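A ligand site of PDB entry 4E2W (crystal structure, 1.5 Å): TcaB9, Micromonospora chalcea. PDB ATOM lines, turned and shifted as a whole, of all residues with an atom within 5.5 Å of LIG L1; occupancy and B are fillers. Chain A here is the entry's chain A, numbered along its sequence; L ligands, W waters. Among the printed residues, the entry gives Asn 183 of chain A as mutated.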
ATOM      1  N   ASP A  35       4.491   2.430  28.777  1.00  0.00           N
ATOM      2  CA  ASP A  35       3.993   3.632  28.143  1.00  0.00           C
ATOM      3  C   ASP A  35       5.039   4.749  28.122  1.00  0.00           C
ATOM      4  O   ASP A  35       4.660   5.900  27.867  1.00  0.00           O
ATOM      5  CB  ASP A  35       2.630   4.081  28.712  1.00  0.00           C
ATOM      6  CG  ASP A  35       1.468   3.444  27.973  1.00  0.00           C
ATOM      7  OD1 ASP A  35       1.453   3.533  26.736  1.00  0.00           O
ATOM      8  OD2 ASP A  35       0.512   2.922  28.585  1.00  0.00           O
ATOM      9  N   TYR A  78       1.811  10.984  30.427  1.00  0.00           N
ATOM     10  CA  TYR A  78       1.221   9.717  29.985  1.00  0.00           C
ATOM     11  C   TYR A  78       0.547   9.811  28.605  1.00  0.00           C
ATOM     12  O   TYR A  78      -0.246  10.751  28.372  1.00  0.00           O
ATOM     13  CB  TYR A  78       0.194   9.339  31.074  1.00  0.00           C
ATOM     14  CG  TYR A  78      -0.459   7.991  30.840  1.00  0.00           C
ATOM     15  CD1 TYR A  78      -1.790   7.918  30.461  1.00  0.00           C
ATOM     16  CD2 TYR A  78       0.244   6.813  31.026  1.00  0.00           C
ATOM     17  CE1 TYR A  78      -2.440   6.682  30.281  1.00  0.00           C
ATOM     18  CE2 TYR A  78      -0.380   5.580  30.829  1.00  0.00           C
ATOM     19  CZ  TYR A  78      -1.719   5.528  30.479  1.00  0.00           C
ATOM     20  OH  TYR A  78      -2.395   4.350  30.258  1.00  0.00           O
ATOM     21  N   TYR A  80      -1.402   7.664  26.546  1.00  0.00           N
ATOM     22  CA  TYR A  80      -2.519   6.932  25.922  1.00  0.00           C
ATOM     23  C   TYR A  80      -3.744   7.829  25.767  1.00  0.00           C
ATOM     24  O   TYR A  80      -4.203   8.434  26.741  1.00  0.00           O
ATOM     25  CB  TYR A  80      -2.966   5.796  26.837  1.00  0.00           C
ATOM     26  CG  TYR A  80      -4.067   4.983  26.191  1.00  0.00           C
ATOM     27  CD1 TYR A  80      -3.841   4.280  25.009  1.00  0.00           C
ATOM     28  CD2 TYR A  80      -5.345   4.939  26.774  1.00  0.00           C
ATOM     29  CE1 TYR A  80      -4.827   3.541  24.347  1.00  0.00           C
ATOM     30  CE2 TYR A  80      -6.353   4.203  26.136  1.00  0.00           C
ATOM     31  CZ  TYR A  80      -6.073   3.525  24.959  1.00  0.00           C
ATOM     32  OH  TYR A  80      -7.025   2.751  24.342  1.00  0.00           O
ATOM     33  N   GLY A  84      -8.623   7.863  20.536  1.00  0.00           N
ATOM     34  CA  GLY A  84      -8.026   7.402  19.295  1.00  0.00           C
ATOM     35  C   GLY A  84      -8.718   6.266  18.583  1.00  0.00           C
ATOM     36  O   GLY A  84      -8.389   5.980  17.429  1.00  0.00           O
ATOM     37  N   SER A  85      -9.729   5.636  19.167  1.00  0.00           N
ATOM     38  CA  SER A  85     -10.448   4.521  18.526  1.00  0.00           C
ATOM     39  C   SER A  85     -11.927   4.883  18.364  1.00  0.00           C
ATOM     40  O   SER A  85     -12.616   5.215  19.345  1.00  0.00           O
ATOM     41  CB  SER A  85     -10.442   3.327  19.481  1.00  0.00           C
ATOM     42  OG  SER A  85     -11.386   2.345  19.066  1.00  0.00           O
ATOM     43  N   SER A  86     -12.422   4.780  17.138  1.00  0.00           N
ATOM     44  CA  SER A  86     -13.852   5.004  16.886  1.00  0.00           C
ATOM     45  C   SER A  86     -14.759   3.977  17.561  1.00  0.00           C
ATOM     46  O   SER A  86     -15.848   4.307  18.059  1.00  0.00           O
ATOM     47  CB  SER A  86     -14.133   5.026  15.382  1.00  0.00           C
ATOM     48  OG  SER A  86     -13.888   3.753  14.800  1.00  0.00           O
ATOM     49  N   ASN A 179     -10.894  -0.004  32.305  1.00  0.00           N
ATOM     50  CA  ASN A 179      -9.448  -0.159  31.992  1.00  0.00           C
ATOM     51  C   ASN A 179      -8.590   0.613  32.999  1.00  0.00           C
ATOM     52  O   ASN A 179      -7.472   1.022  32.634  1.00  0.00           O
ATOM     53  CB  ASN A 179      -9.165   0.204  30.540  1.00  0.00           C
ATOM     54  CG  ASN A 179     -10.117  -0.589  29.653  1.00  0.00           C
ATOM     55  OD1 ASN A 179     -10.099  -1.814  29.762  1.00  0.00           O
ATOM     56  ND2 ASN A 179     -10.994   0.083  28.897  1.00  0.00           N
ATOM     57  N   ASN A 183      -5.569  -1.518  37.136  1.00  0.00           N
ATOM     58  CA  ASN A 183      -4.212  -0.948  37.144  1.00  0.00           C
ATOM     59  C   ASN A 183      -3.822  -0.603  38.586  1.00  0.00           C
ATOM     60  O   ASN A 183      -2.688  -0.170  38.828  1.00  0.00           O
ATOM     61  CB  ASN A 183      -4.159   0.430  36.475  1.00  0.00           C
ATOM     62  CG  ASN A 183      -4.689   0.556  35.087  1.00  0.00           C
ATOM     63  OD1 ASN A 183      -4.506   1.623  34.486  1.00  0.00           O
ATOM     64  ND2 ASN A 183      -5.372  -0.460  34.526  1.00  0.00           N
ATOM     65  N   TYR A 224       1.186  -6.477  31.745  1.00  0.00           N
ATOM     66  CA  TYR A 224       2.224  -5.456  31.657  1.00  0.00           C
ATOM     67  C   TYR A 224       2.066  -4.555  32.878  1.00  0.00           C
ATOM     68  O   TYR A 224       1.145  -4.725  33.684  1.00  0.00           O
ATOM     69  CB  TYR A 224       2.256  -4.688  30.312  1.00  0.00           C
ATOM     70  CG  TYR A 224       1.016  -3.916  29.940  1.00  0.00           C
ATOM     71  CD1 TYR A 224       0.888  -2.549  30.255  1.00  0.00           C
ATOM     72  CD2 TYR A 224      -0.016  -4.564  29.290  1.00  0.00           C
ATOM     73  CE1 TYR A 224      -0.266  -1.827  29.913  1.00  0.00           C
ATOM     74  CE2 TYR A 224      -1.174  -3.869  28.931  1.00  0.00           C
ATOM     75  CZ  TYR A 224      -1.276  -2.529  29.259  1.00  0.00           C
ATOM     76  OH  TYR A 224      -2.385  -1.792  28.952  1.00  0.00           O
ATOM     77  N   GLU A 226       0.888  -1.760  33.825  1.00  0.00           N
ATOM     78  CA  GLU A 226      -0.383  -1.096  34.157  1.00  0.00           C
ATOM     79  C   GLU A 226      -1.544  -2.074  34.381  1.00  0.00           C
ATOM     80  O   GLU A 226      -2.637  -1.640  34.792  1.00  0.00           O
ATOM     81  CB  GLU A 226      -0.740  -0.113  33.021  1.00  0.00           C
ATOM     82  CG  GLU A 226       0.247   1.033  32.898  1.00  0.00           C
ATOM     83  CD  GLU A 226      -0.017   1.840  31.624  1.00  0.00           C
ATOM     84  OE1 GLU A 226      -1.188   1.936  31.183  1.00  0.00           O
ATOM     85  OE2 GLU A 226       0.918   2.469  31.070  1.00  0.00           O
ATOM     86  N   HIS A 227      -1.349  -3.366  34.090  1.00  0.00           N
ATOM     87  CA  HIS A 227      -2.390  -4.311  34.486  1.00  0.00           C
ATOM     88  C   HIS A 227      -2.000  -5.162  35.686  1.00  0.00           C
ATOM     89  O   HIS A 227      -1.457  -6.233  35.507  1.00  0.00           O
ATOM     90  CB  HIS A 227      -2.722  -5.217  33.293  1.00  0.00           C
ATOM     91  CG  HIS A 227      -3.464  -4.452  32.229  1.00  0.00           C
ATOM     92  ND1 HIS A 227      -3.755  -4.988  30.996  1.00  0.00           N
ATOM     93  CD2 HIS A 227      -4.001  -3.207  32.232  1.00  0.00           C
ATOM     94  CE1 HIS A 227      -4.415  -4.103  30.254  1.00  0.00           C
ATOM     95  NE2 HIS A 227      -4.590  -3.023  31.003  1.00  0.00           N
ATOM     96  N   HIS A 256     -11.109  -4.563  23.818  1.00  0.00           N
ATOM     97  CA  HIS A 256      -9.823  -4.837  24.460  1.00  0.00           C
ATOM     98  C   HIS A 256      -9.468  -6.306  24.604  1.00  0.00           C
ATOM     99  O   HIS A 256      -8.829  -6.664  25.596  1.00  0.00           O
ATOM    100  CB  HIS A 256      -9.661  -4.047  25.759  1.00  0.00           C
ATOM    101  CG  HIS A 256      -9.562  -2.568  25.513  1.00  0.00           C
ATOM    102  ND1 HIS A 256      -8.547  -2.011  24.756  1.00  0.00           N
ATOM    103  CD2 HIS A 256     -10.357  -1.544  25.897  1.00  0.00           C
ATOM    104  CE1 HIS A 256      -8.742  -0.710  24.673  1.00  0.00           C
ATOM    105  NE2 HIS A 256      -9.819  -0.398  25.363  1.00  0.00           N
ATOM    106  N   TYR A 325       2.145  -2.682  13.692  1.00  0.00           N
ATOM    107  CA  TYR A 325       1.011  -1.775  13.627  1.00  0.00           C
ATOM    108  C   TYR A 325       0.344  -1.618  14.982  1.00  0.00           C
ATOM    109  O   TYR A 325      -0.192  -2.610  15.530  1.00  0.00           O
ATOM    110  CB  TYR A 325       0.011  -2.202  12.557  1.00  0.00           C
ATOM    111  CG  TYR A 325      -0.809  -1.056  12.028  1.00  0.00           C
ATOM    112  CD1 TYR A 325      -1.702  -0.387  12.867  1.00  0.00           C
ATOM    113  CD2 TYR A 325      -0.703  -0.687  10.672  1.00  0.00           C
ATOM    114  CE1 TYR A 325      -2.481   0.674  12.354  1.00  0.00           C
ATOM    115  CE2 TYR A 325      -1.474   0.366  10.191  1.00  0.00           C
ATOM    116  CZ  TYR A 325      -2.354   1.032  11.027  1.00  0.00           C
ATOM    117  OH  TYR A 325      -3.121   2.082  10.563  1.00  0.00           O
ATOM    118  N   GLY A 326       0.465  -0.397  15.511  1.00  0.00           N
ATOM    119  CA  GLY A 326      -0.093  -0.017  16.811  1.00  0.00           C
ATOM    120  C   GLY A 326       0.995  -0.046  17.872  1.00  0.00           C
ATOM    121  O   GLY A 326       1.466  -1.124  18.260  1.00  0.00           O
ATOM    122  N   ALA A 327       1.392   1.099  18.424  1.00  0.00           N
ATOM    123  CA  ALA A 327       2.388   1.180  19.506  1.00  0.00           C
ATOM    124  C   ALA A 327       1.674   1.024  20.849  1.00  0.00           C
ATOM    125  O   ALA A 327       1.681   1.884  21.757  1.00  0.00           O
ATOM    126  CB  ALA A 327       3.209   2.504  19.423  1.00  0.00           C
ATOM    127  N   THR A 328       1.061  -0.147  20.995  1.00  0.00           N
ATOM    128  CA  THR A 328       0.300  -0.474  22.185  1.00  0.00           C
ATOM    129  C   THR A 328       1.232  -0.529  23.392  1.00  0.00           C
ATOM    130  O   THR A 328       2.415  -0.854  23.261  1.00  0.00           O
ATOM    131  CB  THR A 328      -0.355  -1.870  22.014  1.00  0.00           C
ATOM    132  OG1 THR A 328       0.660  -2.819  21.686  1.00  0.00           O
ATOM    133  CG2 THR A 328      -1.437  -1.798  20.906  1.00  0.00           C
ATOM    134  N   ALA A 329       0.745  -0.228  24.591  1.00  0.00           N
ATOM    135  CA  ALA A 329       1.381  -0.617  25.844  1.00  0.00           C
ATOM    136  C   ALA A 329       1.648  -2.140  25.894  1.00  0.00           C
ATOM    137  O   ALA A 329       2.752  -2.583  26.185  1.00  0.00           O
ATOM    138  CB  ALA A 329       0.593  -0.129  27.062  1.00  0.00           C
ATOM    139  N   LYS A 330       0.643  -2.903  25.449  1.00  0.00           N
ATOM    140  CA  LYS A 330       0.733  -4.363  25.431  1.00  0.00           C
ATOM    141  C   LYS A 330       2.000  -4.838  24.716  1.00  0.00           C
ATOM    142  O   LYS A 330       2.615  -5.833  25.076  1.00  0.00           O
ATOM    143  CB  LYS A 330      -0.531  -4.840  24.684  1.00  0.00           C
ATOM    144  CG  LYS A 330      -1.889  -4.783  25.470  1.00  0.00           C
ATOM    145  CD  LYS A 330      -3.060  -5.583  24.808  1.00  0.00           C
ATOM    146  CE  LYS A 330      -3.264  -5.040  23.397  1.00  0.00           C
ATOM    147  NZ  LYS A 330      -3.941  -3.721  23.344  1.00  0.00           N
ATOM    148  N   TYR A 349       3.838   1.621  13.316  1.00  0.00           N
ATOM    149  CA  TYR A 349       2.968   2.698  12.839  1.00  0.00           C
ATOM    150  C   TYR A 349       1.883   2.949  13.900  1.00  0.00           C
ATOM    151  O   TYR A 349       1.274   2.046  14.477  1.00  0.00           O
ATOM    152  CB  TYR A 349       2.366   2.373  11.438  1.00  0.00           C
ATOM    153  CG  TYR A 349       3.525   2.336  10.472  1.00  0.00           C
ATOM    154  CD1 TYR A 349       4.105   3.510   9.977  1.00  0.00           C
ATOM    155  CD2 TYR A 349       4.118   1.124  10.131  1.00  0.00           C
ATOM    156  CE1 TYR A 349       5.191   3.471   9.130  1.00  0.00           C
ATOM    157  CE2 TYR A 349       5.222   1.078   9.327  1.00  0.00           C
ATOM    158  CZ  TYR A 349       5.742   2.254   8.834  1.00  0.00           C
ATOM    159  OH  TYR A 349       6.848   2.165   8.027  1.00  0.00           O
ATOM    160  N   ASP A 350       1.696   4.224  14.263  1.00  0.00           N
ATOM    161  CA  ASP A 350       0.726   4.558  15.297  1.00  0.00           C
ATOM    162  C   ASP A 350       0.078   5.947  15.144  1.00  0.00           C
ATOM    163  O   ASP A 350       0.763   6.844  14.650  1.00  0.00           O
ATOM    164  CB  ASP A 350       1.428   4.580  16.683  1.00  0.00           C
ATOM    165  CG  ASP A 350       0.466   4.610  17.831  1.00  0.00           C
ATOM    166  OD1 ASP A 350       0.064   3.514  18.314  1.00  0.00           O
ATOM    167  OD2 ASP A 350       0.158   5.729  18.298  1.00  0.00           O
ATOM    168  N   THR A 351      -1.184   6.126  15.540  1.00  0.00           N
ATOM    169  CA  THR A 351      -1.860   7.386  15.287  1.00  0.00           C
ATOM    170  C   THR A 351      -1.660   8.409  16.409  1.00  0.00           C
ATOM    171  O   THR A 351      -2.203   9.511  16.298  1.00  0.00           O
ATOM    172  CB  THR A 351      -3.376   7.209  15.134  1.00  0.00           C
ATOM    173  OG1 THR A 351      -3.835   6.422  16.241  1.00  0.00           O
ATOM    174  CG2 THR A 351      -3.682   6.416  13.843  1.00  0.00           C
ATOM    175  N   THR A 352      -0.957   8.079  17.490  1.00  0.00           N
ATOM    176  CA  THR A 352      -0.787   8.999  18.609  1.00  0.00           C
ATOM    177  C   THR A 352       0.402   9.949  18.458  1.00  0.00           C
ATOM    178  O   THR A 352       1.575   9.548  18.470  1.00  0.00           O
ATOM    179  CB  THR A 352      -0.537   8.219  19.940  1.00  0.00           C
ATOM    180  OG1 THR A 352      -1.361   7.051  19.991  1.00  0.00           O
ATOM    181  CG2 THR A 352      -0.735   9.121  21.153  1.00  0.00           C
ATOM    182  N   LYS A 355       3.512   9.550  20.656  1.00  0.00           N
ATOM    183  CA  LYS A 355       4.332   8.340  20.487  1.00  0.00           C
ATOM    184  C   LYS A 355       5.126   8.360  19.187  1.00  0.00           C
ATOM    185  O   LYS A 355       6.102   7.636  19.025  1.00  0.00           O
ATOM    186  CB  LYS A 355       3.439   7.069  20.452  1.00  0.00           C
ATOM    187  CG  LYS A 355       2.632   6.783  21.734  1.00  0.00           C
ATOM    188  CD  LYS A 355       1.836   5.495  21.553  1.00  0.00           C
ATOM    189  CE  LYS A 355       0.924   5.236  22.761  1.00  0.00           C
ATOM    190  NZ  LYS A 355       0.184   3.946  22.748  1.00  0.00           N
ATOM    191  N   ALA A 370       0.836   6.731  11.401  1.00  0.00           N
ATOM    192  CA  ALA A 370       0.140   5.719  10.584  1.00  0.00           C
ATOM    193  C   ALA A 370      -0.038   6.181   9.132  1.00  0.00           C
ATOM    194  O   ALA A 370      -0.104   5.403   8.176  1.00  0.00           O
ATOM    195  CB  ALA A 370      -1.229   5.401  11.232  1.00  0.00           C
ATOM    196  N   ALA A 385      -1.902  -3.918  17.783  1.00  0.00           N
ATOM    197  CA  ALA A 385      -3.266  -3.506  18.175  1.00  0.00           C
ATOM    198  C   ALA A 385      -4.287  -4.505  17.592  1.00  0.00           C
ATOM    199  O   ALA A 385      -5.227  -4.135  16.914  1.00  0.00           O
ATOM    200  CB  ALA A 385      -3.476  -2.080  17.656  1.00  0.00           C
ATOM    201  N   ASN A 387      -6.535  -6.056  19.180  1.00  0.00           N
ATOM    202  CA  ASN A 387      -7.851  -5.802  19.762  1.00  0.00           C
ATOM    203  C   ASN A 387      -8.639  -4.793  18.955  1.00  0.00           C
ATOM    204  O   ASN A 387      -9.844  -4.639  19.175  1.00  0.00           O
ATOM    205  CB  ASN A 387      -7.762  -5.301  21.222  1.00  0.00           C
ATOM    206  CG  ASN A 387      -6.754  -4.157  21.408  1.00  0.00           C
ATOM    207  OD1 ASN A 387      -5.583  -4.320  21.079  1.00  0.00           O
ATOM    208  ND2 ASN A 387      -7.206  -3.007  21.927  1.00  0.00           N
ATOM    209  N   HIS A 388      -7.979  -4.111  18.034  1.00  0.00           N
ATOM    210  CA  HIS A 388      -8.549  -3.098  17.159  1.00  0.00           C
ATOM    211  C   HIS A 388      -8.544  -3.607  15.712  1.00  0.00           C
ATOM    212  O   HIS A 388      -8.673  -2.818  14.760  1.00  0.00           O
ATOM    213  CB  HIS A 388      -7.774  -1.783  17.218  1.00  0.00           C
ATOM    214  CG  HIS A 388      -7.891  -1.077  18.533  1.00  0.00           C
ATOM    215  ND1 HIS A 388      -9.082  -0.547  18.982  1.00  0.00           N
ATOM    216  CD2 HIS A 388      -6.970  -0.817  19.495  1.00  0.00           C
ATOM    217  CE1 HIS A 388      -8.884   0.046  20.152  1.00  0.00           C
ATOM    218  NE2 HIS A 388      -7.613  -0.130  20.492  1.00  0.00           N
ATOM    219  N   GLU A 391     -11.352  -2.312  13.121  1.00  0.00           N
ATOM    220  CA  GLU A 391     -11.235  -0.874  12.874  1.00  0.00           C
ATOM    221  C   GLU A 391     -10.012  -0.490  12.031  1.00  0.00           C
ATOM    222  O   GLU A 391     -10.068   0.293  11.073  1.00  0.00           O
ATOM    223  CB  GLU A 391     -11.113  -0.153  14.234  1.00  0.00           C
ATOM    224  CG  GLU A 391     -11.107   1.355  14.088  1.00  0.00           C
ATOM    225  CD  GLU A 391     -11.192   2.119  15.402  1.00  0.00           C
ATOM    226  OE1 GLU A 391     -10.821   3.338  15.425  1.00  0.00           O
ATOM    227  OE2 GLU A 391     -11.650   1.493  16.379  1.00  0.00           O
ATOM    228  N   ILE A 392      -8.889  -1.065  12.411  1.00  0.00           N
ATOM    229  CA  ILE A 392      -7.649  -0.901  11.657  1.00  0.00           C
ATOM    230  C   ILE A 392      -7.706  -1.488  10.232  1.00  0.00           C
ATOM    231  O   ILE A 392      -7.417  -0.753   9.275  1.00  0.00           O
ATOM    232  CB  ILE A 392      -6.430  -1.441  12.435  1.00  0.00           C
ATOM    233  CG1 ILE A 392      -6.034  -0.481  13.583  1.00  0.00           C
ATOM    234  CG2 ILE A 392      -5.221  -1.469  11.477  1.00  0.00           C
ATOM    235  CD1 ILE A 392      -5.096  -1.155  14.656  1.00  0.00           C
ATOM    236  N   LYS A 395      -9.507   0.575   7.699  1.00  0.00           N
ATOM    237  CA  LYS A 395      -8.822   1.762   7.207  1.00  0.00           C
ATOM    238  C   LYS A 395      -7.619   1.423   6.348  1.00  0.00           C
ATOM    239  O   LYS A 395      -7.051   2.284   5.698  1.00  0.00           O
ATOM    240  CB  LYS A 395      -8.263   2.560   8.391  1.00  0.00           C
ATOM    241  CG  LYS A 395      -9.316   3.324   9.167  1.00  0.00           C
ATOM    242  CD  LYS A 395      -8.629   4.309  10.108  1.00  0.00           C
ATOM    243  CE  LYS A 395      -8.362   3.591  11.412  1.00  0.00           C
ATOM    244  NZ  LYS A 395      -7.707   4.618  12.284  1.00  0.00           N
HETATM  245  P1  LIG L   1      -4.844   0.116  22.749  1.00  0.00           P
HETATM  246  C1  LIG L   1      -3.581   1.273  26.856  1.00  0.00           C
HETATM  247  O1  LIG L   1      -3.285  -0.059  26.425  1.00  0.00           O
HETATM  248  C2  LIG L   1      -2.880   1.512  28.209  1.00  0.00           C
HETATM  249  P2  LIG L   1      -2.896  -0.245  24.879  1.00  0.00           P
HETATM  250  C3  LIG L   1      -3.957   0.976  29.179  1.00  0.00           C
HETATM  251  N1  LIG L   1      -3.319   0.324  30.327  1.00  0.00           N
HETATM  252  C4  LIG L   1      -5.056   0.043  28.684  1.00  0.00           C
HETATM  253  O2  LIG L   1      -5.461  -0.954  29.267  1.00  0.00           O
HETATM  254  C5  LIG L   1      -5.767   0.324  27.413  1.00  0.00           C
HETATM  255  O3  LIG L   1      -5.014   1.416  26.884  1.00  0.00           O
HETATM  256  C6  LIG L   1      -7.228   0.787  27.474  1.00  0.00           C
HETATM  257  C7  LIG L   1      -2.935   2.871  17.908  1.00  0.00           C
HETATM  258  N2  LIG L   1      -3.994   2.819  16.895  1.00  0.00           N
HETATM  259  O4  LIG L   1      -6.173   0.882  22.784  1.00  0.00           O
HETATM  260  C8  LIG L   1      -3.300   3.886  18.984  1.00  0.00           C
HETATM  261  C9  LIG L   1      -3.725   3.162  15.623  1.00  0.00           C
HETATM  262  O5  LIG L   1      -2.551   3.430  15.275  1.00  0.00           O
HETATM  263  O6  LIG L   1      -4.938  -1.300  22.215  1.00  0.00           O
HETATM  264  C10 LIG L   1      -2.778   3.310  20.290  1.00  0.00           C
HETATM  265  O7  LIG L   1      -1.417   3.749  20.516  1.00  0.00           O
HETATM  266  N3  LIG L   1      -4.710   3.054  14.684  1.00  0.00           N
HETATM  267  C11 LIG L   1      -4.726   2.233  29.607  1.00  0.00           C
HETATM  268  O8  LIG L   1      -2.510  -1.661  24.554  1.00  0.00           O
HETATM  269  C12 LIG L   1      -2.710   1.812  19.973  1.00  0.00           C
HETATM  270  O9  LIG L   1      -2.830   1.615  18.578  1.00  0.00           O
HETATM  271  C13 LIG L   1      -6.002   2.808  14.973  1.00  0.00           C
HETATM  272  O10 LIG L   1      -6.844   2.785  14.049  1.00  0.00           O
HETATM  273  O11 LIG L   1      -1.874   0.804  24.527  1.00  0.00           O
HETATM  274  C14 LIG L   1      -3.868   0.964  20.447  1.00  0.00           C
HETATM  275  O12 LIG L   1      -3.743   0.887  21.866  1.00  0.00           O
HETATM  276  C15 LIG L   1      -6.372   2.421  16.361  1.00  0.00           C
HETATM  277  C16 LIG L   1      -7.780   2.054  16.790  1.00  0.00           C
HETATM  278  C17 LIG L   1      -5.271   2.486  17.216  1.00  0.00           C
HETATM  279  O13 LIG L   1      -4.311   0.239  24.268  1.00  0.00           O
HETATM  280  N1  LG2 L   2     -11.168   4.913  30.899  1.00  0.00           N
HETATM  281  C1  LG2 L   2     -10.215   5.100  29.768  1.00  0.00           C
HETATM  282  C2  LG2 L   2      -8.748   5.265  30.130  1.00  0.00           C
HETATM  283  C3  LG2 L   2      -7.912   4.056  30.514  1.00  0.00           C
HETATM  284  S1  LG2 L   2      -6.229   4.575  30.720  1.00  0.00           S
HETATM  285  C4  LG2 L   2     -10.396   3.979  28.778  1.00  0.00           C
HETATM  286  O1  LG2 L   2     -11.002   2.963  29.162  1.00  0.00           O
HETATM  287  O2  LG2 L   2      -9.920   4.075  27.648  1.00  0.00           O
HETATM  288  C5  LG2 L   2      -6.128   4.381  32.483  1.00  0.00           C
HETATM  289  C6  LG2 L   2      -6.265   5.767  33.119  1.00  0.00           C
HETATM  290  O3  LG2 L   2      -6.288   5.519  34.536  1.00  0.00           O
HETATM  291  C7  LG2 L   2      -5.019   6.602  32.852  1.00  0.00           C
HETATM  292  O4  LG2 L   2      -5.406   7.798  32.161  1.00  0.00           O
HETATM  293  C8  LG2 L   2      -4.479   6.909  34.245  1.00  0.00           C
HETATM  294  O5  LG2 L   2      -3.934   8.225  34.405  1.00  0.00           O
HETATM  295  C9  LG2 L   2      -5.725   6.716  35.109  1.00  0.00           C
HETATM  296  N2  LG2 L   2      -5.472   6.359  36.536  1.00  0.00           N
HETATM  297  C10 LG2 L   2      -4.513   5.592  37.064  1.00  0.00           C
HETATM  298  N3  LG2 L   2      -4.646   5.438  38.406  1.00  0.00           N
HETATM  299  C11 LG2 L   2      -5.788   6.107  38.734  1.00  0.00           C
HETATM  300  C12 LG2 L   2      -6.525   6.366  39.982  1.00  0.00           C
HETATM  301  N4  LG2 L   2      -6.123   5.904  41.183  1.00  0.00           N
HETATM  302  N5  LG2 L   2      -7.600   7.155  39.818  1.00  0.00           N
HETATM  303  C13 LG2 L   2      -8.049   7.667  38.669  1.00  0.00           C
HETATM  304  N6  LG2 L   2      -7.464   7.469  37.493  1.00  0.00           N
HETATM  305  C14 LG2 L   2      -6.333   6.709  37.506  1.00  0.00           C
HETATM  306  O   HOH W   1      -3.943  -2.829  27.118  1.00  0.00           O
HETATM  307  O   HOH W   2      -5.430  -0.325  32.051  1.00  0.00           O
HETATM  308  O   HOH W   3      -4.425   3.836  11.916  1.00  0.00           O
HETATM  309  O   HOH W   4      -5.318   5.781  20.944  1.00  0.00           O
HETATM  310  O   HOH W   5      -0.709   3.221  25.185  1.00  0.00           O
HETATM  311  O   HOH W   6      -6.453   5.982  15.475  1.00  0.00           O
HETATM  312  O   HOH W   7      -7.443  -2.734  29.085  1.00  0.00           O
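Water W7 lies within hydrogen-bond range of O2 of LIG L1, OD1 of Asn 179 and NE2 of His 227.
Water W5 lies within hydrogen-bond range of OD1 of Asp 35, NZ of Lys 355 and O11 of LIG L1.
Water W2 lies within hydrogen-bond range of ND2 of Asn 183 (2.5 Å), O of Asn 179 (2.5 Å), N1 of LIG L1 (2.8 Å) and NE2 of His 227 (3.0 Å).
Water W3 lies within hydrogen-bond range of the side-chain hydroxyl of Tyr 325 (2.6 Å), a nitrogen (N3) of LIG L1 (2.9 Å) and the side-chain amino group of Lys 395 (3.4 Å).
Water W1 lies within hydrogen-bond range of the side-chain hydroxyl of Tyr 224 and an oxygen (O1) of LIG L1.
Water W6 lies within hydrogen-bond range of O of Gly 84, OG1 of Thr 351 and N3 of LIG L1.
Merely in contact with LIG L1: Tyr 78, Thr 328, Ile 392, His 256, Glu 391, Gly 326, Asn 179, Asp 35, Ala 327, Ala 385 and Ser 85.
24 residues have an atom within 4 Å of LIG L1: Asp 35, Tyr 78, Tyr 80, Ser 85, Asn 179, Tyr 224, Glu 226, His 227, His 256, Gly 326, Ala 327, Thr 328, Ala 329, Lys 330, Asp 350, Thr 351, Thr 352, Lys 355, Ala 385, Asn 387, His 388, Glu 391, Ile 392 and Lys 395.
O of Asp 350 sits at hydrogen-bond distance from N of Ala 370, at 3.3 Å.
The side-chain amino group (NZ) of Lys 330 is in hydrogen-bond range of the side-chain amide oxygen (OD1) of Asn 387 (2.9 Å).
OE1 of Glu 226 sits at hydrogen-bond distance from OH of Tyr 78, at 2.9 Å.
The side-chain amino group (NZ) of Lys 355 lies within hydrogen-bond range of the backbone carbonyl oxygen (O) of Ala 327 (2.7 Å).
The backbone carbonyl oxygen (O) of Tyr 349 sits at hydrogen-bond distance from the backbone NH (N) of Gly 326.
The side-chain amide nitrogen (ND2) of Asn 183 lies close to the backbone carbonyl oxygen (O) of Glu 226 (3.0 Å).
The side-chain amide nitrogen (ND2) of Asn 387 lies within hydrogen-bond range of a ring nitrogen (ND1) of His 256 (3.3 Å).
The side-chain carboxylate of Glu 391 sits at hydrogen-bond distance from the backbone NH of Ser 86 (2.8 Å).
An oxygen (O2) of LIG L1 is in hydrogen-bond range of a ring nitrogen (NE2) of His 227.
A ring nitrogen (NE2) of His 388 lies within hydrogen-bond range of an oxygen (O4) of LIG L1 (2.9 Å).
An oxygen (O5) of LIG L1 lies close to the side-chain hydroxyl (OG1) of Thr 351, at 3.4 Å.
N of Ala 329 sits at hydrogen-bond distance from O11 of LIG L1, at 2.8 Å.
NZ of Lys 355 is in hydrogen-bond range of O7 of LIG L1, 2.8 Å away.
N of Thr 351 lies within hydrogen-bond range of O5 of LIG L1 (3.0 Å).
An oxygen (O7) of LIG L1 is in hydrogen-bond range of the side-chain carboxylate (OD1) of Asp 350, 2.7 Å away.
An oxygen (O10) of LIG L1 sits at hydrogen-bond distance from the side-chain amino group (NZ) of Lys 395 (2.7 Å).
OE1 of Glu 226 lies within salt-bridge range of N1 of LIG L1.
OH of Tyr 80 sits at hydrogen-bond distance from O4 of LIG L1 (2.6 Å).
N1 of LIG L1 lies within hydrogen-bond range of OH of Tyr 224 (2.7 Å).
An oxygen (O1) of LG2 L2 is in hydrogen-bond range of the side-chain amide nitrogen (ND2) of Asn 179 (2.9 Å).
An oxygen (O6) of LIG L1 lies within hydrogen-bond range of the side-chain amide nitrogen (ND2) of Asn 387, at 2.9 Å.
The side-chain hydroxyl of Thr 352 lies within hydrogen-bond range of an oxygen (O7) of LIG L1.
An oxygen (O8) of LIG L1 lies within salt-bridge range of the side-chain amino group (NZ) of Lys 330 (2.8 Å).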
